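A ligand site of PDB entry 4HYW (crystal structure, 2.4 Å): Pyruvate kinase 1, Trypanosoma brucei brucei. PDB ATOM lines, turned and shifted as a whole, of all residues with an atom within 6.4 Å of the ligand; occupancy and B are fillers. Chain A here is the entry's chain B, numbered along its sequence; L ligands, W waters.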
ATOM      1  N   VAL A 399      -8.935  26.489  -7.455  1.00  0.00           N
ATOM      2  CA  VAL A 399      -8.990  26.222  -8.875  1.00  0.00           C
ATOM      3  C   VAL A 399     -10.250  26.849  -9.415  1.00  0.00           C
ATOM      4  O   VAL A 399     -11.265  26.905  -8.722  1.00  0.00           O
ATOM      5  CB  VAL A 399      -9.022  24.716  -9.162  1.00  0.00           C
ATOM      6  CG1 VAL A 399     -10.229  24.072  -8.487  1.00  0.00           C
ATOM      7  CG2 VAL A 399      -8.981  24.422 -10.674  1.00  0.00           C
ATOM      8  N   LEU A 400     -10.135  27.455 -10.585  1.00  0.00           N
ATOM      9  CA  LEU A 400     -11.281  28.006 -11.305  1.00  0.00           C
ATOM     10  C   LEU A 400     -11.802  26.961 -12.259  1.00  0.00           C
ATOM     11  O   LEU A 400     -11.047  26.463 -13.131  1.00  0.00           O
ATOM     12  CB  LEU A 400     -10.818  29.217 -12.110  1.00  0.00           C
ATOM     13  CG  LEU A 400     -11.041  30.557 -11.446  1.00  0.00           C
ATOM     14  CD1 LEU A 400     -10.421  30.615 -10.050  1.00  0.00           C
ATOM     15  CD2 LEU A 400     -10.505  31.663 -12.347  1.00  0.00           C
ATOM     16  N   SER A 401     -13.081  26.631 -12.132  1.00  0.00           N
ATOM     17  CA  SER A 401     -13.643  25.605 -12.988  1.00  0.00           C
ATOM     18  C   SER A 401     -15.108  25.870 -13.281  1.00  0.00           C
ATOM     19  O   SER A 401     -15.896  26.104 -12.367  1.00  0.00           O
ATOM     20  CB  SER A 401     -13.449  24.216 -12.367  1.00  0.00           C
ATOM     21  OG  SER A 401     -13.875  23.186 -13.258  1.00  0.00           O
ATOM     22  N   ASN A 402     -15.473  25.845 -14.543  1.00  0.00           N
ATOM     23  CA  ASN A 402     -16.826  26.192 -14.922  1.00  0.00           C
ATOM     24  C   ASN A 402     -17.664  24.950 -15.133  1.00  0.00           C
ATOM     25  O   ASN A 402     -18.805  24.881 -14.662  1.00  0.00           O
ATOM     26  CB  ASN A 402     -16.821  27.115 -16.139  1.00  0.00           C
ATOM     27  CG  ASN A 402     -16.084  28.415 -15.870  1.00  0.00           C
ATOM     28  OD1 ASN A 402     -16.314  29.068 -14.827  1.00  0.00           O
ATOM     29  ND2 ASN A 402     -15.124  28.751 -16.740  1.00  0.00           N
ATOM     30  N   THR A 403     -17.058  23.919 -15.674  1.00  0.00           N
ATOM     31  CA  THR A 403     -17.745  22.662 -15.865  1.00  0.00           C
ATOM     32  C   THR A 403     -17.535  21.701 -14.686  1.00  0.00           C
ATOM     33  O   THR A 403     -18.257  20.709 -14.553  1.00  0.00           O
ATOM     34  CB  THR A 403     -17.270  21.962 -17.124  1.00  0.00           C
ATOM     35  OG1 THR A 403     -15.890  21.598 -16.964  1.00  0.00           O
ATOM     36  CG2 THR A 403     -17.444  22.921 -18.360  1.00  0.00           C
ATOM     37  N   GLY A 404     -16.488  21.935 -13.903  1.00  0.00           N
ATOM     38  CA  GLY A 404     -16.028  20.973 -12.904  1.00  0.00           C
ATOM     39  C   GLY A 404     -14.821  20.151 -13.325  1.00  0.00           C
ATOM     40  O   GLY A 404     -14.134  19.571 -12.475  1.00  0.00           O
ATOM     41  N   ARG A 405     -14.556  20.117 -14.626  1.00  0.00           N
ATOM     42  CA  ARG A 405     -13.503  19.286 -15.204  1.00  0.00           C
ATOM     43  C   ARG A 405     -12.174  19.438 -14.431  1.00  0.00           C
ATOM     44  O   ARG A 405     -11.566  18.442 -14.007  1.00  0.00           O
ATOM     45  CB  ARG A 405     -13.314  19.633 -16.681  1.00  0.00           C
ATOM     46  CG  ARG A 405     -12.596  18.582 -17.505  1.00  0.00           C
ATOM     47  CD  ARG A 405     -12.730  18.856 -19.007  1.00  0.00           C
ATOM     48  NE  ARG A 405     -14.092  18.643 -19.481  1.00  0.00           N
ATOM     49  CZ  ARG A 405     -14.918  19.607 -19.883  1.00  0.00           C
ATOM     50  NH1 ARG A 405     -14.509  20.883 -19.885  1.00  0.00           N
ATOM     51  NH2 ARG A 405     -16.141  19.308 -20.279  1.00  0.00           N
ATOM     52  N   SER A 406     -11.735  20.679 -14.282  1.00  0.00           N
ATOM     53  CA  SER A 406     -10.424  20.979 -13.701  1.00  0.00           C
ATOM     54  C   SER A 406     -10.372  20.687 -12.218  1.00  0.00           C
ATOM     55  O   SER A 406      -9.319  20.299 -11.704  1.00  0.00           O
ATOM     56  CB  SER A 406     -10.064  22.448 -13.914  1.00  0.00           C
ATOM     57  OG  SER A 406      -9.999  22.750 -15.294  1.00  0.00           O
ATOM     58  N   ALA A 407     -11.472  20.926 -11.503  1.00  0.00           N
ATOM     59  CA  ALA A 407     -11.581  20.480 -10.105  1.00  0.00           C
ATOM     60  C   ALA A 407     -11.441  18.968  -9.961  1.00  0.00           C
ATOM     61  O   ALA A 407     -10.742  18.488  -9.076  1.00  0.00           O
ATOM     62  CB  ALA A 407     -12.895  20.958  -9.469  1.00  0.00           C
ATOM     63  N   THR A 424     -18.667  29.233 -12.094  1.00  0.00           N
ATOM     64  CA  THR A 424     -19.708  30.160 -12.562  1.00  0.00           C
ATOM     65  C   THR A 424     -21.066  29.481 -12.753  1.00  0.00           C
ATOM     66  O   THR A 424     -22.001  30.075 -13.316  1.00  0.00           O
ATOM     67  CB  THR A 424     -19.301  30.852 -13.885  1.00  0.00           C
ATOM     68  OG1 THR A 424     -19.138  29.874 -14.905  1.00  0.00           O
ATOM     69  CG2 THR A 424     -18.003  31.618 -13.720  1.00  0.00           C
ATOM     70  N   ARG A 425     -21.199  28.229 -12.301  1.00  0.00           N
ATOM     71  CA  ARG A 425     -22.431  27.454 -12.485  1.00  0.00           C
ATOM     72  C   ARG A 425     -22.856  26.820 -11.181  1.00  0.00           C
ATOM     73  O   ARG A 425     -22.084  26.075 -10.566  1.00  0.00           O
ATOM     74  CB  ARG A 425     -22.218  26.347 -13.527  1.00  0.00           C
ATOM     75  CG  ARG A 425     -21.928  26.861 -14.916  1.00  0.00           C
ATOM     76  CD  ARG A 425     -21.933  25.731 -15.938  1.00  0.00           C
ATOM     77  NE  ARG A 425     -21.253  26.175 -17.152  1.00  0.00           N
ATOM     78  CZ  ARG A 425     -20.893  25.375 -18.157  1.00  0.00           C
ATOM     79  NH1 ARG A 425     -21.198  24.070 -18.145  1.00  0.00           N
ATOM     80  NH2 ARG A 425     -20.245  25.892 -19.196  1.00  0.00           N
ATOM     81  N   ASP A 451     -14.836  38.978 -15.465  1.00  0.00           N
ATOM     82  CA  ASP A 451     -13.629  38.417 -14.820  1.00  0.00           C
ATOM     83  C   ASP A 451     -12.622  37.759 -15.762  1.00  0.00           C
ATOM     84  O   ASP A 451     -12.007  36.752 -15.415  1.00  0.00           O
ATOM     85  CB  ASP A 451     -13.998  37.465 -13.677  1.00  0.00           C
ATOM     86  CG  ASP A 451     -12.897  37.362 -12.637  1.00  0.00           C
ATOM     87  OD1 ASP A 451     -12.214  38.378 -12.425  1.00  0.00           O
ATOM     88  OD2 ASP A 451     -12.701  36.268 -12.036  1.00  0.00           O
ATOM     89  N   LYS A 452     -12.361  38.383 -16.912  1.00  0.00           N
ATOM     90  CA  LYS A 452     -11.422  37.832 -17.885  1.00  0.00           C
ATOM     91  C   LYS A 452     -10.044  37.555 -17.282  1.00  0.00           C
ATOM     92  O   LYS A 452      -9.394  36.582 -17.635  1.00  0.00           O
ATOM     93  CB  LYS A 452     -11.287  38.758 -19.093  1.00  0.00           C
ATOM     94  CG  LYS A 452     -11.877  38.183 -20.376  1.00  0.00           C
ATOM     95  CD  LYS A 452     -11.562  39.051 -21.590  1.00  0.00           C
ATOM     96  CE  LYS A 452     -12.579  38.842 -22.702  1.00  0.00           C
ATOM     97  NZ  LYS A 452     -13.967  38.738 -22.163  1.00  0.00           N
ATOM     98  N   LYS A 454      -9.467  36.891 -14.112  1.00  0.00           N
ATOM     99  CA  LYS A 454      -9.564  35.862 -13.046  1.00  0.00           C
ATOM    100  C   LYS A 454      -9.461  36.467 -11.646  1.00  0.00           C
ATOM    101  O   LYS A 454      -9.683  35.768 -10.650  1.00  0.00           O
ATOM    102  CB  LYS A 454      -8.498  34.737 -13.211  1.00  0.00           C
ATOM    103  CG  LYS A 454      -7.875  34.596 -14.606  1.00  0.00           C
ATOM    104  CD  LYS A 454      -8.784  33.815 -15.531  1.00  0.00           C
ATOM    105  CE  LYS A 454      -8.231  33.802 -16.932  1.00  0.00           C
ATOM    106  NZ  LYS A 454      -9.259  33.339 -17.900  1.00  0.00           N
ATOM    107  N   ARG A 457     -12.553  36.192  -9.253  1.00  0.00           N
ATOM    108  CA  ARG A 457     -12.806  34.819  -8.833  1.00  0.00           C
ATOM    109  C   ARG A 457     -11.747  34.328  -7.867  1.00  0.00           C
ATOM    110  O   ARG A 457     -12.067  33.723  -6.852  1.00  0.00           O
ATOM    111  CB  ARG A 457     -12.962  33.882 -10.018  1.00  0.00           C
ATOM    112  CG  ARG A 457     -14.302  34.039 -10.722  1.00  0.00           C
ATOM    113  CD  ARG A 457     -14.365  33.233 -12.007  1.00  0.00           C
ATOM    114  NE  ARG A 457     -13.590  33.833 -13.080  1.00  0.00           N
ATOM    115  CZ  ARG A 457     -13.195  33.181 -14.171  1.00  0.00           C
ATOM    116  NH1 ARG A 457     -13.477  31.900 -14.337  1.00  0.00           N
ATOM    117  NH2 ARG A 457     -12.508  33.828 -15.106  1.00  0.00           N
ATOM    118  N   VAL A 480      -4.764  27.546  -9.440  1.00  0.00           N
ATOM    119  CA  VAL A 480      -4.722  26.947 -10.746  1.00  0.00           C
ATOM    120  C   VAL A 480      -5.832  27.576 -11.591  1.00  0.00           C
ATOM    121  O   VAL A 480      -6.998  27.613 -11.179  1.00  0.00           O
ATOM    122  CB  VAL A 480      -4.943  25.419 -10.672  1.00  0.00           C
ATOM    123  CG1 VAL A 480      -5.080  24.820 -12.084  1.00  0.00           C
ATOM    124  CG2 VAL A 480      -3.804  24.722  -9.912  1.00  0.00           C
ATOM    125  N   HIS A 481      -5.452  28.168 -12.713  1.00  0.00           N
ATOM    126  CA  HIS A 481      -6.401  28.610 -13.744  1.00  0.00           C
ATOM    127  C   HIS A 481      -5.613  28.939 -14.971  1.00  0.00           C
ATOM    128  O   HIS A 481      -4.469  28.507 -15.109  1.00  0.00           O
ATOM    129  CB  HIS A 481      -7.265  29.822 -13.265  1.00  0.00           C
ATOM    130  CG  HIS A 481      -6.441  31.012 -12.765  1.00  0.00           C
ATOM    131  ND1 HIS A 481      -5.654  31.769 -13.588  1.00  0.00           N
ATOM    132  CD2 HIS A 481      -6.284  31.541 -11.467  1.00  0.00           C
ATOM    133  CE1 HIS A 481      -5.021  32.732 -12.857  1.00  0.00           C
ATOM    134  NE2 HIS A 481      -5.417  32.600 -11.566  1.00  0.00           N
ATOM    135  N   ALA A 482      -6.235  29.616 -15.930  1.00  0.00           N
ATOM    136  CA  ALA A 482      -5.517  29.987 -17.162  1.00  0.00           C
ATOM    137  C   ALA A 482      -4.766  31.305 -17.030  1.00  0.00           C
ATOM    138  O   ALA A 482      -5.084  32.129 -16.176  1.00  0.00           O
ATOM    139  CB  ALA A 482      -6.456  30.011 -18.364  1.00  0.00           C
ATOM    140  N   ASP A 483      -3.766  31.508 -17.883  1.00  0.00           N
ATOM    141  CA  ASP A 483      -3.169  32.828 -17.982  1.00  0.00           C
ATOM    142  C   ASP A 483      -4.114  33.798 -18.708  1.00  0.00           C
ATOM    143  O   ASP A 483      -5.316  33.530 -18.874  1.00  0.00           O
ATOM    144  CB  ASP A 483      -1.775  32.765 -18.636  1.00  0.00           C
ATOM    145  CG  ASP A 483      -1.808  32.278 -20.064  1.00  0.00           C
ATOM    146  OD1 ASP A 483      -2.854  32.465 -20.748  1.00  0.00           O
ATOM    147  OD2 ASP A 483      -0.777  31.724 -20.522  1.00  0.00           O
ATOM    148  N   VAL A 486      -4.911  31.984 -22.812  1.00  0.00           N
ATOM    149  CA  VAL A 486      -5.411  30.634 -23.043  1.00  0.00           C
ATOM    150  C   VAL A 486      -6.878  30.451 -22.591  1.00  0.00           C
ATOM    151  O   VAL A 486      -7.283  30.938 -21.531  1.00  0.00           O
ATOM    152  CB  VAL A 486      -4.491  29.595 -22.404  1.00  0.00           C
ATOM    153  CG1 VAL A 486      -5.122  28.204 -22.423  1.00  0.00           C
ATOM    154  CG2 VAL A 486      -3.118  29.604 -23.092  1.00  0.00           C
ATOM    155  N   LYS A 487      -7.686  29.805 -23.448  1.00  0.00           N
ATOM    156  CA  LYS A 487      -9.117  29.543 -23.159  1.00  0.00           C
ATOM    157  C   LYS A 487      -9.413  28.044 -23.172  1.00  0.00           C
ATOM    158  O   LYS A 487      -8.833  27.310 -23.964  1.00  0.00           O
ATOM    159  CB  LYS A 487     -10.037  30.261 -24.177  1.00  0.00           C
ATOM    160  CG  LYS A 487      -9.775  31.745 -24.305  1.00  0.00           C
ATOM    161  CD  LYS A 487     -10.230  32.508 -23.079  1.00  0.00           C
ATOM    162  CE  LYS A 487      -9.414  33.795 -22.890  1.00  0.00           C
ATOM    163  NZ  LYS A 487      -9.906  34.659 -21.761  1.00  0.00           N
ATOM    164  N   GLY A 488     -10.323  27.610 -22.302  1.00  0.00           N
ATOM    165  CA  GLY A 488     -10.859  26.253 -22.368  1.00  0.00           C
ATOM    166  C   GLY A 488     -10.326  25.264 -21.328  1.00  0.00           C
ATOM    167  O   GLY A 488     -10.878  24.161 -21.175  1.00  0.00           O
ATOM    168  N   TYR A 489      -9.231  25.637 -20.654  1.00  0.00           N
ATOM    169  CA  TYR A 489      -8.533  24.772 -19.678  1.00  0.00           C
ATOM    170  C   TYR A 489      -7.455  25.583 -18.940  1.00  0.00           C
ATOM    171  O   TYR A 489      -7.032  26.617 -19.418  1.00  0.00           O
ATOM    172  CB  TYR A 489      -7.873  23.574 -20.386  1.00  0.00           C
ATOM    173  CG  TYR A 489      -6.722  23.963 -21.311  1.00  0.00           C
ATOM    174  CD1 TYR A 489      -6.965  24.277 -22.666  1.00  0.00           C
ATOM    175  CD2 TYR A 489      -5.412  24.042 -20.843  1.00  0.00           C
ATOM    176  CE1 TYR A 489      -5.910  24.643 -23.514  1.00  0.00           C
ATOM    177  CE2 TYR A 489      -4.354  24.394 -21.675  1.00  0.00           C
ATOM    178  CZ  TYR A 489      -4.603  24.695 -23.011  1.00  0.00           C
ATOM    179  OH  TYR A 489      -3.557  25.026 -23.841  1.00  0.00           O
ATOM    180  N   PRO A 490      -7.010  25.100 -17.781  1.00  0.00           N
ATOM    181  CA  PRO A 490      -6.002  25.830 -17.030  1.00  0.00           C
ATOM    182  C   PRO A 490      -4.594  25.483 -17.481  1.00  0.00           C
ATOM    183  O   PRO A 490      -4.266  24.318 -17.594  1.00  0.00           O
ATOM    184  CB  PRO A 490      -6.232  25.345 -15.596  1.00  0.00           C
ATOM    185  CG  PRO A 490      -6.717  23.937 -15.785  1.00  0.00           C
ATOM    186  CD  PRO A 490      -7.609  24.004 -16.987  1.00  0.00           C
ATOM    187  N   ASN A 491      -3.783  26.489 -17.812  1.00  0.00           N
ATOM    188  CA  ASN A 491      -2.368  26.250 -18.184  1.00  0.00           C
ATOM    189  C   ASN A 491      -1.363  26.823 -17.162  1.00  0.00           C
ATOM    190  O   ASN A 491      -0.166  26.883 -17.444  1.00  0.00           O
ATOM    191  CB  ASN A 491      -2.066  26.813 -19.586  1.00  0.00           C
ATOM    192  CG  ASN A 491      -1.988  28.341 -19.609  1.00  0.00           C
ATOM    193  OD1 ASN A 491      -2.807  29.033 -18.999  1.00  0.00           O
ATOM    194  ND2 ASN A 491      -0.968  28.872 -20.297  1.00  0.00           N
HETATM  195  P1  LIG L   1     -12.016  30.888 -17.630  1.00  0.00           P
HETATM  196  O1  LIG L   1     -11.119  31.769 -16.857  1.00  0.00           O
HETATM  197  O2  LIG L   1     -13.461  30.917 -17.058  1.00  0.00           O
HETATM  198  O3  LIG L   1     -12.096  31.231 -19.226  1.00  0.00           O
HETATM  199  O4  LIG L   1     -10.912  29.400 -20.224  1.00  0.00           O
HETATM  200  C1  LIG L   1      -9.911  29.453 -19.201  1.00  0.00           C
HETATM  201  C2  LIG L   1     -10.425  28.691 -17.994  1.00  0.00           C
HETATM  202  O5  LIG L   1     -11.655  29.265 -17.542  1.00  0.00           O
HETATM  203  C3  LIG L   1      -9.412  28.669 -16.865  1.00  0.00           C
HETATM  204  O6  LIG L   1      -9.369  29.967 -16.245  1.00  0.00           O
HETATM  205  C4  LIG L   1     -10.138  27.699 -15.952  1.00  0.00           C
HETATM  206  O7  LIG L   1      -9.271  27.201 -14.927  1.00  0.00           O
HETATM  207  C5  LIG L   1     -10.519  26.585 -16.939  1.00  0.00           C
HETATM  208  O8  LIG L   1     -10.675  27.266 -18.271  1.00  0.00           O
HETATM  209  C6  LIG L   1     -11.848  26.051 -16.573  1.00  0.00           C
HETATM  210  O9  LIG L   1     -12.161  24.929 -17.398  1.00  0.00           O
HETATM  211  P2  LIG L   1     -13.122  23.820 -16.822  1.00  0.00           P
HETATM  212  O10 LIG L   1     -12.662  23.339 -15.476  1.00  0.00           O
HETATM  213  O11 LIG L   1     -14.597  24.509 -16.775  1.00  0.00           O
HETATM  214  O12 LIG L   1     -13.194  22.675 -17.986  1.00  0.00           O
HETATM  215  O   HOH W   1     -11.794  33.997 -19.707  1.00  0.00           O
HETATM  216  O   HOH W   2     -14.387  30.553 -20.726  1.00  0.00           O
HETATM  217  O   HOH W   3     -11.143  21.950 -19.387  1.00  0.00           O
HETATM  218  O   HOH W   4     -14.832  26.326 -18.551  1.00  0.00           O
HETATM  219  O   HOH W   5     -15.690  32.693 -17.193  1.00  0.00           O
HETATM  220  O   HOH W   6     -12.939  26.922 -19.931  1.00  0.00           O
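His 481 touches the ligand.
O of Val 486 touches C1 of the ligand, at 3.8 Å.
Lys 487 touches the ligand.
Pro 490 touches the ligand.
Of the 25 residues printed, 15 come within 4 Å of the ligand.
The nearest printed residue that does not touch the ligand is Gly 404 (4.3 Å).
The backbone NH (N) of Gly 488 sits at hydrogen-bond distance from an oxygen (O4) of the ligand (2.8 Å).
O of Leu 400 sits at hydrogen-bond distance from O7 of the ligand (2.6 Å).
O2 of the ligand lies within salt-bridge range of NH1 of Arg 457, 2.9 Å away.
The guanidinium group of Arg 405 lies within salt-bridge range of an oxygen (O12) of the ligand (2.9 Å).
O8 of the ligand is in hydrogen-bond range of N of Tyr 489 (3.2 Å).
O11 of the ligand lies within hydrogen-bond range of N of Asn 402, 2.7 Å away.
The side-chain hydroxyl (OG) of Ser 406 lies within hydrogen-bond range of an oxygen (O10) of the ligand (2.7 Å).
An oxygen (O12) of the ligand sits at hydrogen-bond distance from the side-chain hydroxyl (OG1) of Thr 403, 3.1 Å away.
N of Thr 403 lies within hydrogen-bond range of O11 of the ligand.
The side-chain amide nitrogen of Asn 402 sits at hydrogen-bond distance from an oxygen (O2) of the ligand (2.7 Å).
An oxygen (O1) of the ligand is in salt-bridge range of the side-chain amino group of Lys 454 (2.6 Å).
The backbone NH (N) of Ala 482 lies within hydrogen-bond range of an oxygen (O6) of the ligand, at 3.2 Å.
N of Ser 406 sits at hydrogen-bond distance from O10 of the ligand, 3.1 Å away.
The side-chain hydroxyl (OG) of Ser 401 sits at hydrogen-bond distance from an oxygen (O10) of the ligand (2.5 Å).
The backbone carbonyl oxygen (O) of His 481 lies within hydrogen-bond range of the backbone NH (N) of Asn 491 (3.4 Å).
The side-chain hydroxyl (OG1) of Thr 403 lies within hydrogen-bond range of the backbone NH (N) of Arg 405 (3.1 Å).
The backbone NH (N) of Ser 406 is in hydrogen-bond range of the side-chain hydroxyl (OG) of Ser 401.
The side-chain carboxylate of Asp 483 is in hydrogen-bond range of the backbone NH of Val 486, at 3.0 Å.
OG of Ser 401 lies within hydrogen-bond range of N of Arg 405 (3.4 Å).
O of Val 480 sits at hydrogen-bond distance from N of Leu 400 (3.2 Å).
OD1 of Asn 402 is in hydrogen-bond range of OG1 of Thr 424 (2.9 Å).
OD2 of Asp 451 is in salt-bridge range of NE of Arg 457 (2.8 Å).
Water W4 lies within hydrogen-bond range of an oxygen (O11) of the ligand (2.6 Å) and the side-chain amide nitrogen of Asn 402 (3.0 Å).
Water W3 lies within hydrogen-bond range of O12 of the ligand (2.6 Å) and O of Gly 488 (2.9 Å).
Water W1 lies within hydrogen-bond range of O3 of the ligand, NZ of Lys 487 and NZ of Lys 454.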
